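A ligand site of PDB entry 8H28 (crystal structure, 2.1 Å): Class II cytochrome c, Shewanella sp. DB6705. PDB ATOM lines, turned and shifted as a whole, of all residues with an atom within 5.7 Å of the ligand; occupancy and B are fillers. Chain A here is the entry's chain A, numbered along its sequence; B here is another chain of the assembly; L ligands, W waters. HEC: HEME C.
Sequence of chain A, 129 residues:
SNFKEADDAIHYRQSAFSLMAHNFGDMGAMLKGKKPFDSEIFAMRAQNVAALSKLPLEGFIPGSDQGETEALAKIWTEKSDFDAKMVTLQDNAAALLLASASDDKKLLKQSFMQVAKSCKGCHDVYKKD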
ATOM      1  N   ILE A  10      18.957  20.443  24.374  1.00  0.00           N
ATOM      2  CA  ILE A  10      19.964  19.900  23.468  1.00  0.00           C
ATOM      3  C   ILE A  10      21.301  20.618  23.691  1.00  0.00           C
ATOM      4  O   ILE A  10      22.333  19.987  23.943  1.00  0.00           O
ATOM      5  CB  ILE A  10      19.489  20.005  22.012  1.00  0.00           C
ATOM      6  CG1 ILE A  10      18.281  19.087  21.783  1.00  0.00           C
ATOM      7  CG2 ILE A  10      20.602  19.611  21.040  1.00  0.00           C
ATOM      8  CD1 ILE A  10      17.591  19.297  20.448  1.00  0.00           C
ATOM      9  N   ARG A  13      23.014  19.498  27.089  1.00  0.00           N
ATOM     10  CA  ARG A  13      23.638  18.180  27.100  1.00  0.00           C
ATOM     11  C   ARG A  13      24.831  18.132  26.144  1.00  0.00           C
ATOM     12  O   ARG A  13      25.849  17.503  26.448  1.00  0.00           O
ATOM     13  CB  ARG A  13      22.586  17.104  26.785  1.00  0.00           C
ATOM     14  CG  ARG A  13      22.055  17.064  25.354  1.00  0.00           C
ATOM     15  CD  ARG A  13      20.695  16.361  25.313  1.00  0.00           C
ATOM     16  NE  ARG A  13      20.304  15.993  23.959  1.00  0.00           N
ATOM     17  CZ  ARG A  13      19.045  15.878  23.526  1.00  0.00           C
ATOM     18  NH1 ARG A  13      18.015  16.115  24.341  1.00  0.00           N
ATOM     19  NH2 ARG A  13      18.828  15.507  22.267  1.00  0.00           N
ATOM     20  N   GLN A  14      24.727  18.792  24.993  1.00  0.00           N
ATOM     21  CA  GLN A  14      25.860  18.850  24.074  1.00  0.00           C
ATOM     22  C   GLN A  14      27.057  19.586  24.707  1.00  0.00           C
ATOM     23  O   GLN A  14      28.206  19.148  24.575  1.00  0.00           O
ATOM     24  CB  GLN A  14      25.421  19.524  22.769  1.00  0.00           C
ATOM     25  CG  GLN A  14      24.558  18.631  21.846  1.00  0.00           C
ATOM     26  CD  GLN A  14      24.089  19.373  20.588  1.00  0.00           C
ATOM     27  OE1 GLN A  14      24.125  20.600  20.530  1.00  0.00           O
ATOM     28  NE2 GLN A  14      23.610  18.620  19.601  1.00  0.00           N
ATOM     29  N   SER A  15      26.818  20.700  25.388  1.00  0.00           N
ATOM     30  CA  SER A  15      27.919  21.400  26.037  1.00  0.00           C
ATOM     31  C   SER A  15      28.619  20.527  27.070  1.00  0.00           C
ATOM     32  O   SER A  15      29.847  20.478  27.119  1.00  0.00           O
ATOM     33  CB  SER A  15      27.416  22.688  26.695  1.00  0.00           C
ATOM     34  OG  SER A  15      27.150  23.653  25.712  1.00  0.00           O
ATOM     35  N   PHE A  17      28.755  17.181  27.262  1.00  0.00           N
ATOM     36  CA  PHE A  17      29.580  16.190  26.577  1.00  0.00           C
ATOM     37  C   PHE A  17      30.824  16.834  25.991  1.00  0.00           C
ATOM     38  O   PHE A  17      31.919  16.249  26.018  1.00  0.00           O
ATOM     39  CB  PHE A  17      28.788  15.504  25.461  1.00  0.00           C
ATOM     40  CG  PHE A  17      27.718  14.543  25.956  1.00  0.00           C
ATOM     41  CD1 PHE A  17      28.031  13.492  26.814  1.00  0.00           C
ATOM     42  CD2 PHE A  17      26.408  14.657  25.500  1.00  0.00           C
ATOM     43  CE1 PHE A  17      27.035  12.601  27.239  1.00  0.00           C
ATOM     44  CE2 PHE A  17      25.410  13.789  25.917  1.00  0.00           C
ATOM     45  CZ  PHE A  17      25.724  12.756  26.792  1.00  0.00           C
ATOM     46  N   SER A  18      30.682  18.023  25.429  1.00  0.00           N
ATOM     47  CA  SER A  18      31.806  18.703  24.802  1.00  0.00           C
ATOM     48  C   SER A  18      32.900  19.005  25.817  1.00  0.00           C
ATOM     49  O   SER A  18      34.087  18.809  25.528  1.00  0.00           O
ATOM     50  CB  SER A  18      31.311  19.969  24.126  1.00  0.00           C
ATOM     51  OG  SER A  18      32.377  20.655  23.501  1.00  0.00           O
ATOM     52  N   MET A  20      33.298  17.461  28.635  1.00  0.00           N
ATOM     53  CA  MET A  20      33.796  16.167  29.090  1.00  0.00           C
ATOM     54  C   MET A  20      34.868  15.642  28.145  1.00  0.00           C
ATOM     55  O   MET A  20      35.919  15.169  28.592  1.00  0.00           O
ATOM     56  CB  MET A  20      32.645  15.170  29.237  1.00  0.00           C
ATOM     57  CG  MET A  20      32.983  14.021  30.146  1.00  0.00           C
ATOM     58  SD  MET A  20      31.552  13.086  30.713  1.00  0.00           S
ATOM     59  CE  MET A  20      30.640  12.983  29.175  1.00  0.00           C
ATOM     60  N   ALA A  21      34.613  15.740  26.834  1.00  0.00           N
ATOM     61  CA  ALA A  21      35.564  15.261  25.838  1.00  0.00           C
ATOM     62  C   ALA A  21      36.900  15.962  25.948  1.00  0.00           C
ATOM     63  O   ALA A  21      37.964  15.320  25.905  1.00  0.00           O
ATOM     64  CB  ALA A  21      35.003  15.440  24.431  1.00  0.00           C
ATOM     65  N   PHE A  24      38.478  14.490  29.127  1.00  0.00           N
ATOM     66  CA  PHE A  24      38.842  13.087  28.920  1.00  0.00           C
ATOM     67  C   PHE A  24      40.007  12.958  27.938  1.00  0.00           C
ATOM     68  O   PHE A  24      40.957  12.207  28.195  1.00  0.00           O
ATOM     69  CB  PHE A  24      37.605  12.320  28.447  1.00  0.00           C
ATOM     70  CG  PHE A  24      37.789  10.836  28.445  1.00  0.00           C
ATOM     71  CD1 PHE A  24      38.065  10.170  29.639  1.00  0.00           C
ATOM     72  CD2 PHE A  24      37.661  10.112  27.274  1.00  0.00           C
ATOM     73  CE1 PHE A  24      38.239   8.799  29.648  1.00  0.00           C
ATOM     74  CE2 PHE A  24      37.824   8.756  27.278  1.00  0.00           C
ATOM     75  CZ  PHE A  24      38.110   8.085  28.466  1.00  0.00           C
ATOM     76  N   VAL A  49      35.950  15.181  34.872  1.00  0.00           N
ATOM     77  CA  VAL A  49      35.158  14.230  34.112  1.00  0.00           C
ATOM     78  C   VAL A  49      34.022  13.664  34.964  1.00  0.00           C
ATOM     79  O   VAL A  49      32.877  13.616  34.533  1.00  0.00           O
ATOM     80  CB  VAL A  49      36.060  13.111  33.551  1.00  0.00           C
ATOM     81  CG1 VAL A  49      35.207  11.971  32.969  1.00  0.00           C
ATOM     82  CG2 VAL A  49      36.955  13.714  32.486  1.00  0.00           C
ATOM     83  N   PHE A  60      18.061  15.346  28.467  1.00  0.00           N
ATOM     84  CA  PHE A  60      17.327  14.394  27.622  1.00  0.00           C
ATOM     85  C   PHE A  60      15.835  14.386  27.984  1.00  0.00           C
ATOM     86  O   PHE A  60      15.265  13.381  28.404  1.00  0.00           O
ATOM     87  CB  PHE A  60      17.955  13.011  27.727  1.00  0.00           C
ATOM     88  CG  PHE A  60      19.290  12.961  27.074  1.00  0.00           C
ATOM     89  CD1 PHE A  60      19.383  12.762  25.701  1.00  0.00           C
ATOM     90  CD2 PHE A  60      20.424  13.232  27.793  1.00  0.00           C
ATOM     91  CE1 PHE A  60      20.591  12.774  25.080  1.00  0.00           C
ATOM     92  CE2 PHE A  60      21.655  13.251  27.177  1.00  0.00           C
ATOM     93  CZ  PHE A  60      21.744  13.012  25.815  1.00  0.00           C
ATOM     94  N   GLU A  68      18.308  20.210  16.649  1.00  0.00           N
ATOM     95  CA  GLU A  68      19.711  20.199  16.239  1.00  0.00           C
ATOM     96  C   GLU A  68      20.470  19.203  17.122  1.00  0.00           C
ATOM     97  O   GLU A  68      21.290  19.563  17.957  1.00  0.00           O
ATOM     98  CB  GLU A  68      20.291  21.601  16.356  1.00  0.00           C
ATOM     99  CG  GLU A  68      20.057  22.446  15.112  1.00  0.00           C
ATOM    100  CD  GLU A  68      20.196  21.647  13.823  1.00  0.00           C
ATOM    101  OE1 GLU A  68      21.240  20.979  13.642  1.00  0.00           O
ATOM    102  OE2 GLU A  68      19.273  21.714  12.981  1.00  0.00           O
ATOM    103  N   THR A  69      20.214  17.916  16.885  1.00  0.00           N
ATOM    104  CA  THR A  69      20.764  16.904  17.755  1.00  0.00           C
ATOM    105  C   THR A  69      21.218  15.695  16.942  1.00  0.00           C
ATOM    106  O   THR A  69      20.733  15.458  15.828  1.00  0.00           O
ATOM    107  CB  THR A  69      19.729  16.474  18.811  1.00  0.00           C
ATOM    108  OG1 THR A  69      20.290  15.484  19.681  1.00  0.00           O
ATOM    109  CG2 THR A  69      18.460  15.910  18.152  1.00  0.00           C
ATOM    110  N   GLU A  70      22.209  14.991  17.501  1.00  0.00           N
ATOM    111  CA  GLU A  70      22.650  13.687  17.029  1.00  0.00           C
ATOM    112  C   GLU A  70      22.085  12.543  17.862  1.00  0.00           C
ATOM    113  O   GLU A  70      22.431  11.393  17.623  1.00  0.00           O
ATOM    114  CB  GLU A  70      24.189  13.594  17.044  1.00  0.00           C
ATOM    115  CG  GLU A  70      24.953  14.601  16.167  1.00  0.00           C
ATOM    116  CD  GLU A  70      24.584  14.482  14.685  1.00  0.00           C
ATOM    117  OE1 GLU A  70      24.640  13.366  14.119  1.00  0.00           O
ATOM    118  OE2 GLU A  70      24.281  15.523  14.059  1.00  0.00           O
ATOM    119  N   ALA A  71      21.232  12.837  18.850  1.00  0.00           N
ATOM    120  CA  ALA A  71      20.687  11.792  19.696  1.00  0.00           C
ATOM    121  C   ALA A  71      19.613  10.997  18.955  1.00  0.00           C
ATOM    122  O   ALA A  71      18.794  11.576  18.233  1.00  0.00           O
ATOM    123  CB  ALA A  71      20.116  12.380  20.978  1.00  0.00           C
ATOM    124  N   LEU A  72      19.627   9.676  19.106  1.00  0.00           N
ATOM    125  CA  LEU A  72      18.612   8.861  18.457  1.00  0.00           C
ATOM    126  C   LEU A  72      17.325   8.860  19.271  1.00  0.00           C
ATOM    127  O   LEU A  72      17.348   8.790  20.505  1.00  0.00           O
ATOM    128  CB  LEU A  72      19.113   7.436  18.293  1.00  0.00           C
ATOM    129  CG  LEU A  72      20.128   7.217  17.184  1.00  0.00           C
ATOM    130  CD1 LEU A  72      20.735   5.799  17.219  1.00  0.00           C
ATOM    131  CD2 LEU A  72      19.453   7.479  15.847  1.00  0.00           C
ATOM    132  N   ILE A  75      16.609   6.604  22.354  1.00  0.00           N
ATOM    133  CA  ILE A  75      16.896   6.909  23.748  1.00  0.00           C
ATOM    134  C   ILE A  75      15.629   6.866  24.588  1.00  0.00           C
ATOM    135  O   ILE A  75      15.621   6.357  25.706  1.00  0.00           O
ATOM    136  CB  ILE A  75      17.611   8.268  23.878  1.00  0.00           C
ATOM    137  CG1 ILE A  75      19.017   8.174  23.293  1.00  0.00           C
ATOM    138  CG2 ILE A  75      17.752   8.607  25.358  1.00  0.00           C
ATOM    139  CD1 ILE A  75      19.671   9.514  23.188  1.00  0.00           C
ATOM    140  N   PHE A  82      19.393   3.510  28.699  1.00  0.00           N
ATOM    141  CA  PHE A  82      20.209   4.698  28.513  1.00  0.00           C
ATOM    142  C   PHE A  82      20.585   5.218  29.895  1.00  0.00           C
ATOM    143  O   PHE A  82      21.708   5.487  30.126  1.00  0.00           O
ATOM    144  CB  PHE A  82      19.454   5.746  27.718  1.00  0.00           C
ATOM    145  CG  PHE A  82      20.181   7.028  27.463  1.00  0.00           C
ATOM    146  CD1 PHE A  82      20.998   7.164  26.368  1.00  0.00           C
ATOM    147  CD2 PHE A  82      19.985   8.129  28.264  1.00  0.00           C
ATOM    148  CE1 PHE A  82      21.631   8.328  26.110  1.00  0.00           C
ATOM    149  CE2 PHE A  82      20.607   9.299  28.012  1.00  0.00           C
ATOM    150  CZ  PHE A  82      21.426   9.402  26.935  1.00  0.00           C
ATOM    151  N   LYS A  85      23.257   3.200  31.417  1.00  0.00           N
ATOM    152  CA  LYS A  85      24.554   3.473  30.808  1.00  0.00           C
ATOM    153  C   LYS A  85      25.174   4.754  31.352  1.00  0.00           C
ATOM    154  O   LYS A  85      26.399   4.841  31.529  1.00  0.00           O
ATOM    155  CB  LYS A  85      24.435   3.550  29.288  1.00  0.00           C
ATOM    156  CG  LYS A  85      24.110   2.198  28.609  1.00  0.00           C
ATOM    157  CD  LYS A  85      24.288   2.257  27.100  1.00  0.00           C
ATOM    158  CE  LYS A  85      23.914   0.925  26.395  1.00  0.00           C
ATOM    159  NZ  LYS A  85      24.462  -0.312  27.015  1.00  0.00           N
ATOM    160  N   MET A  86      24.347   5.779  31.612  1.00  0.00           N
ATOM    161  CA  MET A  86      24.866   7.023  32.180  1.00  0.00           C
ATOM    162  C   MET A  86      25.399   6.794  33.582  1.00  0.00           C
ATOM    163  O   MET A  86      26.453   7.332  33.958  1.00  0.00           O
ATOM    164  CB  MET A  86      23.788   8.121  32.195  1.00  0.00           C
ATOM    165  CG  MET A  86      24.338   9.565  32.316  1.00  0.00           C
ATOM    166  SD  MET A  86      25.332  10.094  30.899  1.00  0.00           S
ATOM    167  CE  MET A  86      24.031  10.505  29.729  1.00  0.00           C
ATOM    168  N   LEU A  89      28.713   5.149  33.443  1.00  0.00           N
ATOM    169  CA  LEU A  89      29.761   6.129  33.144  1.00  0.00           C
ATOM    170  C   LEU A  89      30.185   6.867  34.405  1.00  0.00           C
ATOM    171  O   LEU A  89      31.379   7.088  34.633  1.00  0.00           O
ATOM    172  CB  LEU A  89      29.285   7.124  32.076  1.00  0.00           C
ATOM    173  CG  LEU A  89      30.167   8.366  31.943  1.00  0.00           C
ATOM    174  CD1 LEU A  89      31.515   7.983  31.287  1.00  0.00           C
ATOM    175  CD2 LEU A  89      29.473   9.461  31.137  1.00  0.00           C
ATOM    176  N   VAL A 115      36.341   3.864  31.217  1.00  0.00           N
ATOM    177  CA  VAL A 115      35.515   5.004  30.953  1.00  0.00           C
ATOM    178  C   VAL A 115      35.298   5.111  29.452  1.00  0.00           C
ATOM    179  O   VAL A 115      34.217   5.341  29.022  1.00  0.00           O
ATOM    180  CB  VAL A 115      36.146   6.280  31.490  1.00  0.00           C
ATOM    181  CG1 VAL A 115      35.347   7.467  31.063  1.00  0.00           C
ATOM    182  CG2 VAL A 115      36.253   6.191  33.000  1.00  0.00           C
ATOM    183  N   SER A 118      32.498   3.085  28.038  1.00  0.00           N
ATOM    184  CA  SER A 118      31.244   3.701  28.329  1.00  0.00           C
ATOM    185  C   SER A 118      30.903   4.774  27.340  1.00  0.00           C
ATOM    186  O   SER A 118      29.804   4.840  26.894  1.00  0.00           O
ATOM    187  CB  SER A 118      31.246   4.312  29.719  1.00  0.00           C
ATOM    188  OG  SER A 118      30.985   3.360  30.691  1.00  0.00           O
ATOM    189  N   CYS A 119      31.855   5.624  26.997  1.00  0.00           N
ATOM    190  CA  CYS A 119      31.564   6.651  26.026  1.00  0.00           C
ATOM    191  C   CYS A 119      31.185   6.000  24.707  1.00  0.00           C
ATOM    192  O   CYS A 119      30.164   6.287  24.159  1.00  0.00           O
ATOM    193  CB  CYS A 119      32.733   7.603  25.795  1.00  0.00           C
ATOM    194  SG  CYS A 119      33.588   8.330  27.176  1.00  0.00           S
ATOM    195  N   LYS A 120      32.032   5.107  24.227  1.00  0.00           N
ATOM    196  CA  LYS A 120      31.827   4.443  22.975  1.00  0.00           C
ATOM    197  C   LYS A 120      30.630   3.542  22.926  1.00  0.00           C
ATOM    198  O   LYS A 120      29.968   3.483  21.938  1.00  0.00           O
ATOM    199  CB  LYS A 120      33.049   3.662  22.552  1.00  0.00           C
ATOM    200  CG  LYS A 120      32.998   3.279  21.080  1.00  0.00           C
ATOM    201  CD  LYS A 120      34.190   2.490  20.623  1.00  0.00           C
ATOM    202  CE  LYS A 120      34.051   2.131  19.164  1.00  0.00           C
ATOM    203  NZ  LYS A 120      33.605   0.722  19.056  1.00  0.00           N
ATOM    204  N   CYS A 122      27.844   3.824  24.591  1.00  0.00           N
ATOM    205  CA  CYS A 122      26.602   4.585  24.481  1.00  0.00           C
ATOM    206  C   CYS A 122      26.483   5.225  23.101  1.00  0.00           C
ATOM    207  O   CYS A 122      25.394   5.236  22.515  1.00  0.00           O
ATOM    208  CB  CYS A 122      26.527   5.650  25.575  1.00  0.00           C
ATOM    209  SG  CYS A 122      24.945   6.522  25.547  1.00  0.00           S
ATOM    210  N   HIS A 123      27.585   5.784  22.586  1.00  0.00           N
ATOM    211  CA  HIS A 123      27.558   6.383  21.265  1.00  0.00           C
ATOM    212  C   HIS A 123      27.147   5.375  20.196  1.00  0.00           C
ATOM    213  O   HIS A 123      26.382   5.711  19.279  1.00  0.00           O
ATOM    214  CB  HIS A 123      28.932   6.981  20.952  1.00  0.00           C
ATOM    215  CG  HIS A 123      29.269   8.172  21.791  1.00  0.00           C
ATOM    216  ND1 HIS A 123      30.553   8.681  21.882  1.00  0.00           N
ATOM    217  CD2 HIS A 123      28.506   8.951  22.582  1.00  0.00           C
ATOM    218  CE1 HIS A 123      30.551   9.719  22.690  1.00  0.00           C
ATOM    219  NE2 HIS A 123      29.323   9.908  23.132  1.00  0.00           N
ATOM    220  N   TYR A 126      23.218   4.906  20.741  1.00  0.00           N
ATOM    221  CA  TYR A 126      22.276   5.996  20.958  1.00  0.00           C
ATOM    222  C   TYR A 126      22.649   7.302  20.287  1.00  0.00           C
ATOM    223  O   TYR A 126      21.894   8.275  20.374  1.00  0.00           O
ATOM    224  CB  TYR A 126      22.075   6.235  22.466  1.00  0.00           C
ATOM    225  CG  TYR A 126      21.398   5.086  23.181  1.00  0.00           C
ATOM    226  CD1 TYR A 126      20.076   4.778  22.914  1.00  0.00           C
ATOM    227  CD2 TYR A 126      22.083   4.294  24.117  1.00  0.00           C
ATOM    228  CE1 TYR A 126      19.442   3.736  23.549  1.00  0.00           C
ATOM    229  CE2 TYR A 126      21.455   3.249  24.767  1.00  0.00           C
ATOM    230  CZ  TYR A 126      20.119   2.975  24.475  1.00  0.00           C
ATOM    231  OH  TYR A 126      19.455   1.930  25.091  1.00  0.00           O
ATOM    232  N   LYS A 127      23.785   7.368  19.588  1.00  0.00           N
ATOM    233  CA  LYS A 127      24.158   8.547  18.837  1.00  0.00           C
ATOM    234  C   LYS A 127      24.134   8.187  17.363  1.00  0.00           C
ATOM    235  O   LYS A 127      24.595   7.109  16.985  1.00  0.00           O
ATOM    236  CB  LYS A 127      25.553   9.037  19.267  1.00  0.00           C
ATOM    237  CG  LYS A 127      25.920  10.435  18.819  1.00  0.00           C
ATOM    238  CD  LYS A 127      27.238  10.871  19.440  1.00  0.00           C
ATOM    239  CE  LYS A 127      27.684  12.241  18.938  1.00  0.00           C
ATOM    240  NZ  LYS A 127      28.243  12.222  17.550  1.00  0.00           N
ATOM    241  N   HIS B  11      34.715  28.312  22.602  1.00  0.00           N
ATOM    242  CA  HIS B  11      33.557  27.436  22.787  1.00  0.00           C
ATOM    243  C   HIS B  11      33.612  26.705  24.117  1.00  0.00           C
ATOM    244  O   HIS B  11      32.600  26.556  24.812  1.00  0.00           O
ATOM    245  CB  HIS B  11      33.463  26.441  21.629  1.00  0.00           C
ATOM    246  CG  HIS B  11      32.329  25.454  21.766  1.00  0.00           C
ATOM    247  ND1 HIS B  11      32.466  24.241  22.402  1.00  0.00           N
ATOM    248  CD2 HIS B  11      31.036  25.515  21.354  1.00  0.00           C
ATOM    249  CE1 HIS B  11      31.318  23.593  22.361  1.00  0.00           C
ATOM    250  NE2 HIS B  11      30.429  24.351  21.736  1.00  0.00           N
HETATM  251 FE   HEC L   1      28.605  11.199  24.438  1.00  0.00          FE
HETATM  252  CHA HEC L   1      27.350  13.618  22.268  1.00  0.00           C
HETATM  253  CHB HEC L   1      31.748  12.855  24.242  1.00  0.00           C
HETATM  254  CHC HEC L   1      29.763   9.416  27.077  1.00  0.00           C
HETATM  255  CHD HEC L   1      25.531   9.855  24.801  1.00  0.00           C
HETATM  256  NA  HEC L   1      29.394  12.930  23.480  1.00  0.00           N
HETATM  257  C1A HEC L   1      28.688  13.682  22.558  1.00  0.00           C
HETATM  258  C2A HEC L   1      29.617  14.580  21.912  1.00  0.00           C
HETATM  259  C3A HEC L   1      30.819  14.400  22.454  1.00  0.00           C
HETATM  260  C4A HEC L   1      30.713  13.344  23.448  1.00  0.00           C
HETATM  261  CMA HEC L   1      32.105  15.164  22.044  1.00  0.00           C
HETATM  262  CAA HEC L   1      29.237  15.614  20.841  1.00  0.00           C
HETATM  263  CBA HEC L   1      28.755  16.814  21.658  1.00  0.00           C
HETATM  264  CGA HEC L   1      28.419  18.004  20.796  1.00  0.00           C
HETATM  265  O1A HEC L   1      29.255  18.945  20.765  1.00  0.00           O
HETATM  266  O2A HEC L   1      27.325  18.022  20.149  1.00  0.00           O
HETATM  267  NB  HEC L   1      30.451  11.198  25.517  1.00  0.00           N
HETATM  268  C1B HEC L   1      31.621  11.868  25.217  1.00  0.00           C
HETATM  269  C2B HEC L   1      32.657  11.350  26.100  1.00  0.00           C
HETATM  270  C3B HEC L   1      32.104  10.386  26.878  1.00  0.00           C
HETATM  271  C4B HEC L   1      30.694  10.285  26.522  1.00  0.00           C
HETATM  272  CMB HEC L   1      34.146  11.791  26.096  1.00  0.00           C
HETATM  273  CAB HEC L   1      32.791   9.511  27.949  1.00  0.00           C
HETATM  274  CBB HEC L   1      33.496  10.326  29.067  1.00  0.00           C
HETATM  275  NC  HEC L   1      27.786   9.891  25.698  1.00  0.00           N
HETATM  276  C1C HEC L   1      28.442   9.226  26.707  1.00  0.00           C
HETATM  277  C2C HEC L   1      27.485   8.365  27.380  1.00  0.00           C
HETATM  278  C3C HEC L   1      26.313   8.434  26.722  1.00  0.00           C
HETATM  279  C4C HEC L   1      26.487   9.426  25.669  1.00  0.00           C
HETATM  280  CMC HEC L   1      27.895   7.366  28.490  1.00  0.00           C
HETATM  281  CAC HEC L   1      24.986   7.637  26.930  1.00  0.00           C
HETATM  282  CBC HEC L   1      24.580   7.171  28.353  1.00  0.00           C
HETATM  283  ND  HEC L   1      26.721  11.699  23.674  1.00  0.00           N
HETATM  284  C1D HEC L   1      25.598  10.924  23.930  1.00  0.00           C
HETATM  285  C2D HEC L   1      24.494  11.393  23.124  1.00  0.00           C
HETATM  286  C3D HEC L   1      25.072  12.572  22.332  1.00  0.00           C
HETATM  287  C4D HEC L   1      26.450  12.684  22.730  1.00  0.00           C
HETATM  288  CMD HEC L   1      23.065  10.819  23.085  1.00  0.00           C
HETATM  289  CAD HEC L   1      24.332  13.460  21.326  1.00  0.00           C
HETATM  290  CBD HEC L   1      23.627  14.551  22.122  1.00  0.00           C
HETATM  291  CGD HEC L   1      22.889  15.468  21.173  1.00  0.00           C
HETATM  292  O1D HEC L   1      23.370  15.669  20.019  1.00  0.00           O
HETATM  293  O2D HEC L   1      21.812  16.020  21.570  1.00  0.00           O
HETATM  294  O   HOH W   1      26.023  15.801  19.768  1.00  0.00           O
HETATM  295  O   HOH W   2      32.053  18.677  21.057  1.00  0.00           O
HETATM  296  O   HOH W   3      26.967  19.876  18.153  1.00  0.00           O
HETATM  297  O   HOH W   4      28.839  21.914  22.348  1.00  0.00           O
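An oxygen (O2D) of the ligand is in hydrogen-bond range of the side-chain hydroxyl (OG1) of Thr 69 (2.5 Å). A carbon (CAB) of the ligand is bonded to the side-chain sulfur of Cys 119 (1.6 Å). An oxygen (O1D) of the ligand is in hydrogen-bond range of the side-chain amide nitrogen (NE2) of Gln 14, 3.0 Å away. N of Glu 70 is in hydrogen-bond range of O1D of the ligand (2.9 Å). The guanidinium group (NE) of Arg 13 lies within salt-bridge range of an oxygen (O2D) of the ligand. The side-chain sulfur (SG) of Cys 122 is bonded to a carbon (CAC) of the ligand, 1.8 Å away. A ring nitrogen (NE2) of His 123 binds an iron atom (FE) of the ligand (2.0 Å).
The backbone NH (N) of Leu 72 is in hydrogen-bond range of the backbone carbonyl oxygen (O) of Tyr 126 (3.0 Å). NH2 of Arg 13 is in hydrogen-bond range of OG1 of Thr 69, 3.0 Å away. The backbone carbonyl oxygen of Cys 119 sits close to a ring nitrogen (ND1) of His 123 (3.3 Å). The side-chain amide nitrogen (NE2) of Gln 14 lies within hydrogen-bond range of the backbone carbonyl oxygen (O) of Glu 68 (3.0 Å). The backbone NH of Ala 71 sits at hydrogen-bond distance from the side-chain hydroxyl of Thr 69 (2.9 Å).
Residues that only touch the ligand: Ile 10, Phe 17, Met 20, Ala 21, Phe 60, Ala 71, Ile 75, Phe 82, Lys 85, Met 86, Leu 89, Val 115, Ser 118, Tyr 126 and Lys 127. 22 residues have an atom within 4 Å of the ligand: Ile 10, Arg 13, Gln 14, Phe 17, Met 20, Ala 21, Phe 60, Thr 69, Glu 70, Ala 71, Ile 75, Phe 82, Lys 85, Met 86, Leu 89, Val 115, Ser 118, Cys 119, Cys 122, His 123, Tyr 126 and Lys 127. The nearest printed residue that does not touch the ligand is Phe 24 (4.1 Å).
Water W2 lies within hydrogen-bond range of an oxygen (O1A) of the ligand and the side-chain hydroxyl of Ser 18. Water W4 lies within hydrogen-bond range of a ring nitrogen (NE2) of His 11 of chain B (3.0 Å) and an oxygen (O1A) of the ligand (3.4 Å).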
